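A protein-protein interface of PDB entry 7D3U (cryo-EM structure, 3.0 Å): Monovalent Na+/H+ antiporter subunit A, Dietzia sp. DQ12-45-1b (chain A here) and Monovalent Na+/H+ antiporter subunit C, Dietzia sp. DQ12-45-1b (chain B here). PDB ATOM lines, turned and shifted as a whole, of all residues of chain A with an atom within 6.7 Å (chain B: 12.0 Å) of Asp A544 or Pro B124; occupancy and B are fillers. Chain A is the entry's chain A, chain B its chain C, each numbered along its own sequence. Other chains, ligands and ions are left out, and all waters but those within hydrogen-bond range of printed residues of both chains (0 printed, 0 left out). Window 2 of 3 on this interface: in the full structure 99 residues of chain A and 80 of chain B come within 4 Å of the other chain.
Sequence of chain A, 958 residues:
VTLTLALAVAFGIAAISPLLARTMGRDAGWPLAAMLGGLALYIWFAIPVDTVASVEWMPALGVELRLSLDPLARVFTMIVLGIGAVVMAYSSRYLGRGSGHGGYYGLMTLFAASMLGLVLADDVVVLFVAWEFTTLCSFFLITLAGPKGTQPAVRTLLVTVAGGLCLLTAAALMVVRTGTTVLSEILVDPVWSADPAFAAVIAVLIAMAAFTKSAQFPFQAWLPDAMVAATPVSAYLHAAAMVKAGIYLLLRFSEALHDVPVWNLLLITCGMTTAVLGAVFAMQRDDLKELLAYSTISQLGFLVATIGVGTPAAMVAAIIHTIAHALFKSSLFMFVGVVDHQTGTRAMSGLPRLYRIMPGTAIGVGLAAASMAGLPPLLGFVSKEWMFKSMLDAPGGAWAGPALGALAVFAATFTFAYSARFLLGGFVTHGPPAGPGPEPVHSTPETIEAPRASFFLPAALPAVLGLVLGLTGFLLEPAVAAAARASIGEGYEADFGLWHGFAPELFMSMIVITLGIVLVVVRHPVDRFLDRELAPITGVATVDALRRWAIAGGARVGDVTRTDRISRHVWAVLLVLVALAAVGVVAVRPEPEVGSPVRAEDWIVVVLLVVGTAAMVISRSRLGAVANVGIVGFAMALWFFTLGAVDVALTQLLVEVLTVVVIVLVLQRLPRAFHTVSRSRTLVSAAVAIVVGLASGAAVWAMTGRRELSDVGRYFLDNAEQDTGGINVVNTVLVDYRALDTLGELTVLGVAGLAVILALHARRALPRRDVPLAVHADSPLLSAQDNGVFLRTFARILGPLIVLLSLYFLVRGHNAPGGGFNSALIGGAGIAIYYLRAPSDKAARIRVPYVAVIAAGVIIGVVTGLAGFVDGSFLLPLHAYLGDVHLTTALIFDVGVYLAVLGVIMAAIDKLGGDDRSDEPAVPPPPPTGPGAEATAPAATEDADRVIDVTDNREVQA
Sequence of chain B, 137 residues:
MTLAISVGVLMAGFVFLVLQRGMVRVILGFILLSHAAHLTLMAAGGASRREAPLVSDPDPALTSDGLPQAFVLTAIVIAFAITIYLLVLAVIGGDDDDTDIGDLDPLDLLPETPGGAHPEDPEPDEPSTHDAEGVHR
Among the printed residues, pairs that only touch across the chains: Gln A151 with Pro B124 (3.5 Å), Asp A544 with Pro B124 (3.3 Å), Arg A547 with Asp B125 (3.3 Å), Arg A548 with Asp B125 (3.3 Å) and Arg A548 with Pro B127 (3.9 Å).
Printed residues of chain B within 4 Å of Gln A151: Glu B123 (3.5 Å) and Pro B124 (3.5 Å). No residue of chain B comes within 4 Å of Val A540. Ala A541 touches none of the printed residues of chain B. Of chain B, only Pro B124 comes within 4 Å of Asp A544. Arg A548 touches three residues of chain B. Printed residues of chain A within 4 Å of Glu B123: Gln A151. Of chain A, only Gln A151 (3.5 Å), Asp A544 (3.3 Å) and Arg A548 (3.2 Å) come within 4 Å of Pro B124. Printed residues of chain A within 4 Å of Pro B127: Arg A548. The nearest residue of chain B that does not touch Asp A544 is Asp B125 (4.3 Å). The nearest printed residue of chain A that does not touch Glu B123 is Arg A547 (5.4 Å).
The side-chain carboxylate (OE1) of Glu B123 sits close to the side-chain amide oxygen (OE1) of Gln A151 (3.5 Å). NH2 of Arg A548 is in hydrogen-bond range of O of Pro B124 (3.2 Å).
NH2 of Arg A547 sits close to NE2 of Gln A151, at 2.9 Å. NH1 of Arg A155 is in salt-bridge range of OD2 of Asp A544 (2.4 Å). NH1 of Arg A547 lies within salt-bridge range of OD1 of Asp A544 (2.9 Å).
Of the 13 printed residues of chain B, 4 touch a printed residue of chain A. Printed residues of chain B that touch a printed residue of chain A: Glu B123, Pro B124, Asp B125 and Pro B127. Of the 13 printed residues of chain A, 4 touch a printed residue of chain B. Printed residues of chain A that touch a printed residue of chain B: Gln A151, Asp A544, Arg A547 and Arg A548.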
ATOM      1  N   GLN A 151     -24.888  -7.371  -8.014  1.00  0.00           N
ATOM      2  CA  GLN A 151     -24.550  -7.553  -6.609  1.00  0.00           C
ATOM      3  C   GLN A 151     -25.794  -7.445  -5.730  1.00  0.00           C
ATOM      4  O   GLN A 151     -25.977  -8.280  -4.833  1.00  0.00           O
ATOM      5  CB  GLN A 151     -23.481  -6.549  -6.175  1.00  0.00           C
ATOM      6  CG  GLN A 151     -22.459  -7.126  -5.222  1.00  0.00           C
ATOM      7  CD  GLN A 151     -21.666  -8.250  -5.846  1.00  0.00           C
ATOM      8  OE1 GLN A 151     -21.238  -8.158  -6.995  1.00  0.00           O
ATOM      9  NE2 GLN A 151     -21.470  -9.323  -5.094  1.00  0.00           N
ATOM     10  N   ARG A 155     -27.165 -10.417  -3.197  1.00  0.00           N
ATOM     11  CA  ARG A 155     -27.451 -10.211  -1.782  1.00  0.00           C
ATOM     12  C   ARG A 155     -28.915 -10.483  -1.466  1.00  0.00           C
ATOM     13  O   ARG A 155     -29.232 -11.045  -0.414  1.00  0.00           O
ATOM     14  CB  ARG A 155     -27.059  -8.795  -1.372  1.00  0.00           C
ATOM     15  CG  ARG A 155     -25.576  -8.538  -1.500  1.00  0.00           C
ATOM     16  CD  ARG A 155     -25.191  -7.217  -0.884  1.00  0.00           C
ATOM     17  NE  ARG A 155     -25.470  -6.097  -1.774  1.00  0.00           N
ATOM     18  CZ  ARG A 155     -24.535  -5.342  -2.338  1.00  0.00           C
ATOM     19  NH1 ARG A 155     -23.254  -5.586  -2.104  1.00  0.00           N
ATOM     20  NH2 ARG A 155     -24.880  -4.342  -3.137  1.00  0.00           N
ATOM     21  N   ASP A 225     -31.334  -1.444  -1.942  1.00  0.00           N
ATOM     22  CA  ASP A 225     -30.469  -1.561  -3.110  1.00  0.00           C
ATOM     23  C   ASP A 225     -31.108  -2.331  -4.256  1.00  0.00           C
ATOM     24  O   ASP A 225     -30.792  -2.059  -5.421  1.00  0.00           O
ATOM     25  CB  ASP A 225     -29.135  -2.217  -2.732  1.00  0.00           C
ATOM     26  CG  ASP A 225     -29.310  -3.584  -2.115  1.00  0.00           C
ATOM     27  OD1 ASP A 225     -30.465  -3.997  -1.904  1.00  0.00           O
ATOM     28  OD2 ASP A 225     -28.288  -4.246  -1.842  1.00  0.00           O
ATOM     29  N   VAL A 540     -25.672  -1.637   3.305  1.00  0.00           N
ATOM     30  CA  VAL A 540     -25.524  -3.025   2.887  1.00  0.00           C
ATOM     31  C   VAL A 540     -24.169  -3.606   3.265  1.00  0.00           C
ATOM     32  O   VAL A 540     -23.904  -4.779   2.970  1.00  0.00           O
ATOM     33  CB  VAL A 540     -25.771  -3.140   1.369  1.00  0.00           C
ATOM     34  CG1 VAL A 540     -24.507  -2.808   0.588  1.00  0.00           C
ATOM     35  CG2 VAL A 540     -26.303  -4.514   1.019  1.00  0.00           C
ATOM     36  N   ALA A 541     -23.314  -2.837   3.937  1.00  0.00           N
ATOM     37  CA  ALA A 541     -21.977  -3.290   4.298  1.00  0.00           C
ATOM     38  C   ALA A 541     -21.963  -4.257   5.476  1.00  0.00           C
ATOM     39  O   ALA A 541     -20.883  -4.559   5.993  1.00  0.00           O
ATOM     40  CB  ALA A 541     -21.082  -2.090   4.613  1.00  0.00           C
ATOM     41  N   THR A 542     -23.121  -4.747   5.914  1.00  0.00           N
ATOM     42  CA  THR A 542     -23.173  -5.775   6.946  1.00  0.00           C
ATOM     43  C   THR A 542     -23.412  -7.166   6.383  1.00  0.00           C
ATOM     44  O   THR A 542     -22.991  -8.151   6.996  1.00  0.00           O
ATOM     45  CB  THR A 542     -24.270  -5.459   7.966  1.00  0.00           C
ATOM     46  OG1 THR A 542     -24.516  -6.614   8.778  1.00  0.00           O
ATOM     47  CG2 THR A 542     -25.553  -5.060   7.258  1.00  0.00           C
ATOM     48  N   VAL A 543     -24.078  -7.269   5.233  1.00  0.00           N
ATOM     49  CA  VAL A 543     -24.200  -8.555   4.560  1.00  0.00           C
ATOM     50  C   VAL A 543     -22.934  -8.860   3.772  1.00  0.00           C
ATOM     51  O   VAL A 543     -22.452  -9.998   3.763  1.00  0.00           O
ATOM     52  CB  VAL A 543     -25.444  -8.568   3.656  1.00  0.00           C
ATOM     53  CG1 VAL A 543     -25.596  -9.921   2.986  1.00  0.00           C
ATOM     54  CG2 VAL A 543     -26.686  -8.218   4.455  1.00  0.00           C
ATOM     55  N   ASP A 544     -22.376  -7.849   3.103  1.00  0.00           N
ATOM     56  CA  ASP A 544     -21.113  -8.038   2.403  1.00  0.00           C
ATOM     57  C   ASP A 544     -19.990  -8.372   3.371  1.00  0.00           C
ATOM     58  O   ASP A 544     -19.087  -9.142   3.028  1.00  0.00           O
ATOM     59  CB  ASP A 544     -20.762  -6.790   1.594  1.00  0.00           C
ATOM     60  CG  ASP A 544     -21.483  -6.737   0.263  1.00  0.00           C
ATOM     61  OD1 ASP A 544     -21.085  -7.475  -0.663  1.00  0.00           O
ATOM     62  OD2 ASP A 544     -22.442  -5.949   0.137  1.00  0.00           O
ATOM     63  N   ALA A 545     -20.030  -7.819   4.585  1.00  0.00           N
ATOM     64  CA  ALA A 545     -19.043  -8.189   5.593  1.00  0.00           C
ATOM     65  C   ALA A 545     -19.168  -9.660   5.966  1.00  0.00           C
ATOM     66  O   ALA A 545     -18.160 -10.353   6.139  1.00  0.00           O
ATOM     67  CB  ALA A 545     -19.195  -7.307   6.830  1.00  0.00           C
ATOM     68  N   LEU A 546     -20.400 -10.159   6.074  1.00  0.00           N
ATOM     69  CA  LEU A 546     -20.596 -11.569   6.393  1.00  0.00           C
ATOM     70  C   LEU A 546     -20.125 -12.461   5.251  1.00  0.00           C
ATOM     71  O   LEU A 546     -19.506 -13.505   5.487  1.00  0.00           O
ATOM     72  CB  LEU A 546     -22.065 -11.831   6.716  1.00  0.00           C
ATOM     73  CG  LEU A 546     -22.463 -13.276   7.005  1.00  0.00           C
ATOM     74  CD1 LEU A 546     -21.746 -13.773   8.247  1.00  0.00           C
ATOM     75  CD2 LEU A 546     -23.967 -13.406   7.169  1.00  0.00           C
ATOM     76  N   ARG A 547     -20.405 -12.067   4.008  1.00  0.00           N
ATOM     77  CA  ARG A 547     -19.924 -12.845   2.870  1.00  0.00           C
ATOM     78  C   ARG A 547     -18.403 -12.844   2.808  1.00  0.00           C
ATOM     79  O   ARG A 547     -17.785 -13.870   2.499  1.00  0.00           O
ATOM     80  CB  ARG A 547     -20.515 -12.298   1.573  1.00  0.00           C
ATOM     81  CG  ARG A 547     -22.029 -12.268   1.552  1.00  0.00           C
ATOM     82  CD  ARG A 547     -22.535 -11.402   0.421  1.00  0.00           C
ATOM     83  NE  ARG A 547     -21.852 -11.711  -0.828  1.00  0.00           N
ATOM     84  CZ  ARG A 547     -21.807 -10.899  -1.876  1.00  0.00           C
ATOM     85  NH1 ARG A 547     -22.405  -9.718  -1.831  1.00  0.00           N
ATOM     86  NH2 ARG A 547     -21.161 -11.270  -2.970  1.00  0.00           N
ATOM     87  N   ARG A 548     -17.780 -11.703   3.104  1.00  0.00           N
ATOM     88  CA  ARG A 548     -16.325 -11.631   3.114  1.00  0.00           C
ATOM     89  C   ARG A 548     -15.740 -12.499   4.220  1.00  0.00           C
ATOM     90  O   ARG A 548     -14.718 -13.163   4.018  1.00  0.00           O
ATOM     91  CB  ARG A 548     -15.876 -10.180   3.272  1.00  0.00           C
ATOM     92  CG  ARG A 548     -14.406 -10.011   3.600  1.00  0.00           C
ATOM     93  CD  ARG A 548     -14.079  -8.565   3.919  1.00  0.00           C
ATOM     94  NE  ARG A 548     -14.541  -7.663   2.870  1.00  0.00           N
ATOM     95  CZ  ARG A 548     -15.498  -6.757   3.035  1.00  0.00           C
ATOM     96  NH1 ARG A 548     -16.096  -6.630   4.210  1.00  0.00           N
ATOM     97  NH2 ARG A 548     -15.857  -5.978   2.024  1.00  0.00           N
ATOM     98  N   TRP A 549     -16.378 -12.515   5.391  1.00  0.00           N
ATOM     99  CA  TRP A 549     -15.920 -13.389   6.466  1.00  0.00           C
ATOM    100  C   TRP A 549     -16.049 -14.853   6.072  1.00  0.00           C
ATOM    101  O   TRP A 549     -15.162 -15.662   6.365  1.00  0.00           O
ATOM    102  CB  TRP A 549     -16.706 -13.114   7.745  1.00  0.00           C
ATOM    103  CG  TRP A 549     -16.562 -14.199   8.763  1.00  0.00           C
ATOM    104  CD1 TRP A 549     -15.445 -14.504   9.481  1.00  0.00           C
ATOM    105  CD2 TRP A 549     -17.568 -15.133   9.170  1.00  0.00           C
ATOM    106  NE1 TRP A 549     -15.693 -15.566  10.315  1.00  0.00           N
ATOM    107  CE2 TRP A 549     -16.991 -15.971  10.143  1.00  0.00           C
ATOM    108  CE3 TRP A 549     -18.902 -15.340   8.809  1.00  0.00           C
ATOM    109  CZ2 TRP A 549     -17.699 -16.999  10.757  1.00  0.00           C
ATOM    110  CZ3 TRP A 549     -19.604 -16.362   9.421  1.00  0.00           C
ATOM    111  CH2 TRP A 549     -19.002 -17.177  10.384  1.00  0.00           C
ATOM    112  N   GLY B 115      -6.701  -7.474 -12.386  1.00  0.00           N
ATOM    113  CA  GLY B 115      -7.945  -6.773 -12.146  1.00  0.00           C
ATOM    114  C   GLY B 115      -9.172  -7.572 -12.532  1.00  0.00           C
ATOM    115  O   GLY B 115     -10.210  -7.488 -11.869  1.00  0.00           O
ATOM    116  N   HIS B 118     -13.383  -6.990 -15.526  1.00  0.00           N
ATOM    117  CA  HIS B 118     -14.045  -5.743 -15.146  1.00  0.00           C
ATOM    118  C   HIS B 118     -13.271  -5.118 -13.997  1.00  0.00           C
ATOM    119  O   HIS B 118     -13.628  -5.276 -12.824  1.00  0.00           O
ATOM    120  CB  HIS B 118     -15.505  -5.986 -14.759  1.00  0.00           C
ATOM    121  CG  HIS B 118     -16.419  -6.161 -15.930  1.00  0.00           C
ATOM    122  ND1 HIS B 118     -16.627  -5.170 -16.865  1.00  0.00           N
ATOM    123  CD2 HIS B 118     -17.182  -7.210 -16.316  1.00  0.00           C
ATOM    124  CE1 HIS B 118     -17.478  -5.602 -17.778  1.00  0.00           C
ATOM    125  NE2 HIS B 118     -17.831  -6.837 -17.468  1.00  0.00           N
ATOM    126  N   PRO B 119     -12.190  -4.394 -14.301  1.00  0.00           N
ATOM    127  CA  PRO B 119     -11.408  -3.757 -13.231  1.00  0.00           C
ATOM    128  C   PRO B 119     -12.113  -2.579 -12.583  1.00  0.00           C
ATOM    129  O   PRO B 119     -11.602  -2.050 -11.588  1.00  0.00           O
ATOM    130  CB  PRO B 119     -10.134  -3.309 -13.953  1.00  0.00           C
ATOM    131  CG  PRO B 119     -10.575  -3.082 -15.356  1.00  0.00           C
ATOM    132  CD  PRO B 119     -11.641  -4.106 -15.637  1.00  0.00           C
ATOM    133  N   GLU B 120     -13.260  -2.154 -13.109  1.00  0.00           N
ATOM    134  CA  GLU B 120     -13.992  -1.026 -12.551  1.00  0.00           C
ATOM    135  C   GLU B 120     -14.979  -1.440 -11.470  1.00  0.00           C
ATOM    136  O   GLU B 120     -15.334  -0.617 -10.619  1.00  0.00           O
ATOM    137  CB  GLU B 120     -14.739  -0.284 -13.661  1.00  0.00           C
ATOM    138  CG  GLU B 120     -15.656  -1.170 -14.486  1.00  0.00           C
ATOM    139  CD  GLU B 120     -15.057  -1.536 -15.829  1.00  0.00           C
ATOM    140  OE1 GLU B 120     -13.875  -1.208 -16.064  1.00  0.00           O
ATOM    141  OE2 GLU B 120     -15.768  -2.152 -16.652  1.00  0.00           O
ATOM    142  N   ASP B 121     -15.434  -2.695 -11.484  1.00  0.00           N
ATOM    143  CA  ASP B 121     -16.422  -3.202 -10.535  1.00  0.00           C
ATOM    144  C   ASP B 121     -15.810  -4.362  -9.757  1.00  0.00           C
ATOM    145  O   ASP B 121     -16.054  -5.536 -10.079  1.00  0.00           O
ATOM    146  CB  ASP B 121     -17.701  -3.635 -11.249  1.00  0.00           C
ATOM    147  CG  ASP B 121     -18.769  -4.126 -10.289  1.00  0.00           C
ATOM    148  OD1 ASP B 121     -18.782  -3.668  -9.127  1.00  0.00           O
ATOM    149  OD2 ASP B 121     -19.595  -4.969 -10.698  1.00  0.00           O
ATOM    150  N   PRO B 122     -15.008  -4.077  -8.732  1.00  0.00           N
ATOM    151  CA  PRO B 122     -14.483  -5.159  -7.894  1.00  0.00           C
ATOM    152  C   PRO B 122     -15.582  -5.756  -7.030  1.00  0.00           C
ATOM    153  O   PRO B 122     -16.417  -5.041  -6.473  1.00  0.00           O
ATOM    154  CB  PRO B 122     -13.416  -4.464  -7.045  1.00  0.00           C
ATOM    155  CG  PRO B 122     -13.866  -3.050  -6.977  1.00  0.00           C
ATOM    156  CD  PRO B 122     -14.521  -2.757  -8.299  1.00  0.00           C
ATOM    157  N   GLU B 123     -15.578  -7.080  -6.931  1.00  0.00           N
ATOM    158  CA  GLU B 123     -16.596  -7.768  -6.152  1.00  0.00           C
ATOM    159  C   GLU B 123     -16.466  -7.393  -4.679  1.00  0.00           C
ATOM    160  O   GLU B 123     -15.374  -7.509  -4.109  1.00  0.00           O
ATOM    161  CB  GLU B 123     -16.470  -9.280  -6.326  1.00  0.00           C
ATOM    162  CG  GLU B 123     -16.585  -9.749  -7.766  1.00  0.00           C
ATOM    163  CD  GLU B 123     -17.999 -10.149  -8.137  1.00  0.00           C
ATOM    164  OE1 GLU B 123     -18.636  -9.422  -8.929  1.00  0.00           O
ATOM    165  OE2 GLU B 123     -18.474 -11.189  -7.635  1.00  0.00           O
ATOM    166  N   PRO B 124     -17.543  -6.939  -4.031  1.00  0.00           N
ATOM    167  CA  PRO B 124     -17.461  -6.584  -2.607  1.00  0.00           C
ATOM    168  C   PRO B 124     -17.323  -7.779  -1.679  1.00  0.00           C
ATOM    169  O   PRO B 124     -17.186  -7.582  -0.466  1.00  0.00           O
ATOM    170  CB  PRO B 124     -18.787  -5.848  -2.351  1.00  0.00           C
ATOM    171  CG  PRO B 124     -19.333  -5.522  -3.710  1.00  0.00           C
ATOM    172  CD  PRO B 124     -18.860  -6.617  -4.601  1.00  0.00           C
ATOM    173  N   ASP B 125     -17.356  -9.003  -2.200  1.00  0.00           N
ATOM    174  CA  ASP B 125     -17.248 -10.190  -1.364  1.00  0.00           C
ATOM    175  C   ASP B 125     -15.808 -10.623  -1.132  1.00  0.00           C
ATOM    176  O   ASP B 125     -15.505 -11.192  -0.077  1.00  0.00           O
ATOM    177  CB  ASP B 125     -18.030 -11.347  -1.991  1.00  0.00           C
ATOM    178  N   GLU B 126     -14.920 -10.369  -2.082  1.00  0.00           N
ATOM    179  CA  GLU B 126     -13.541 -10.822  -1.951  1.00  0.00           C
ATOM    180  C   GLU B 126     -12.824 -10.019  -0.872  1.00  0.00           C
ATOM    181  O   GLU B 126     -12.930  -8.788  -0.850  1.00  0.00           O
ATOM    182  CB  GLU B 126     -12.810 -10.689  -3.284  1.00  0.00           C
ATOM    183  CG  GLU B 126     -13.573 -11.261  -4.471  1.00  0.00           C
ATOM    184  CD  GLU B 126     -13.341 -12.749  -4.664  1.00  0.00           C
ATOM    185  OE1 GLU B 126     -13.606 -13.251  -5.777  1.00  0.00           O
ATOM    186  OE2 GLU B 126     -12.890 -13.416  -3.710  1.00  0.00           O
ATOM    187  N   PRO B 127     -12.089 -10.670   0.036  1.00  0.00           N
ATOM    188  CA  PRO B 127     -11.394  -9.931   1.100  1.00  0.00           C
ATOM    189  C   PRO B 127     -10.201  -9.126   0.620  1.00  0.00           C
ATOM    190  O   PRO B 127      -9.556  -8.462   1.439  1.00  0.00           O
ATOM    191  CB  PRO B 127     -10.948 -11.043   2.069  1.00  0.00           C
ATOM    192  CG  PRO B 127     -11.659 -12.290   1.619  1.00  0.00           C
ATOM    193  CD  PRO B 127     -11.896 -12.121   0.159  1.00  0.00           C
ATOM    194  N   SER B 128      -9.882  -9.160  -0.674  1.00  0.00           N
ATOM    195  CA  SER B 128      -8.759  -8.419  -1.227  1.00  0.00           C
ATOM    196  C   SER B 128      -9.127  -6.986  -1.597  1.00  0.00           C
ATOM    197  O   SER B 128      -8.417  -6.358  -2.389  1.00  0.00           O
ATOM    198  CB  SER B 128      -8.198  -9.150  -2.448  1.00  0.00           C
ATOM    199  OG  SER B 128      -8.124 -10.547  -2.215  1.00  0.00           O
ATOM    200  N   THR B 129     -10.216  -6.461  -1.043  1.00  0.00           N
ATOM    201  CA  THR B 129     -10.643  -5.098  -1.329  1.00  0.00           C
ATOM    202  C   THR B 129     -10.454  -4.200  -0.111  1.00  0.00           C
ATOM    203  O   THR B 129     -10.929  -4.511   0.980  1.00  0.00           O
ATOM    204  CB  THR B 129     -12.117  -5.048  -1.768  1.00  0.00           C
ATOM    205  OG1 THR B 129     -12.431  -6.223  -2.524  1.00  0.00           O
ATOM    206  CG2 THR B 129     -12.377  -3.818  -2.620  1.00  0.00           C
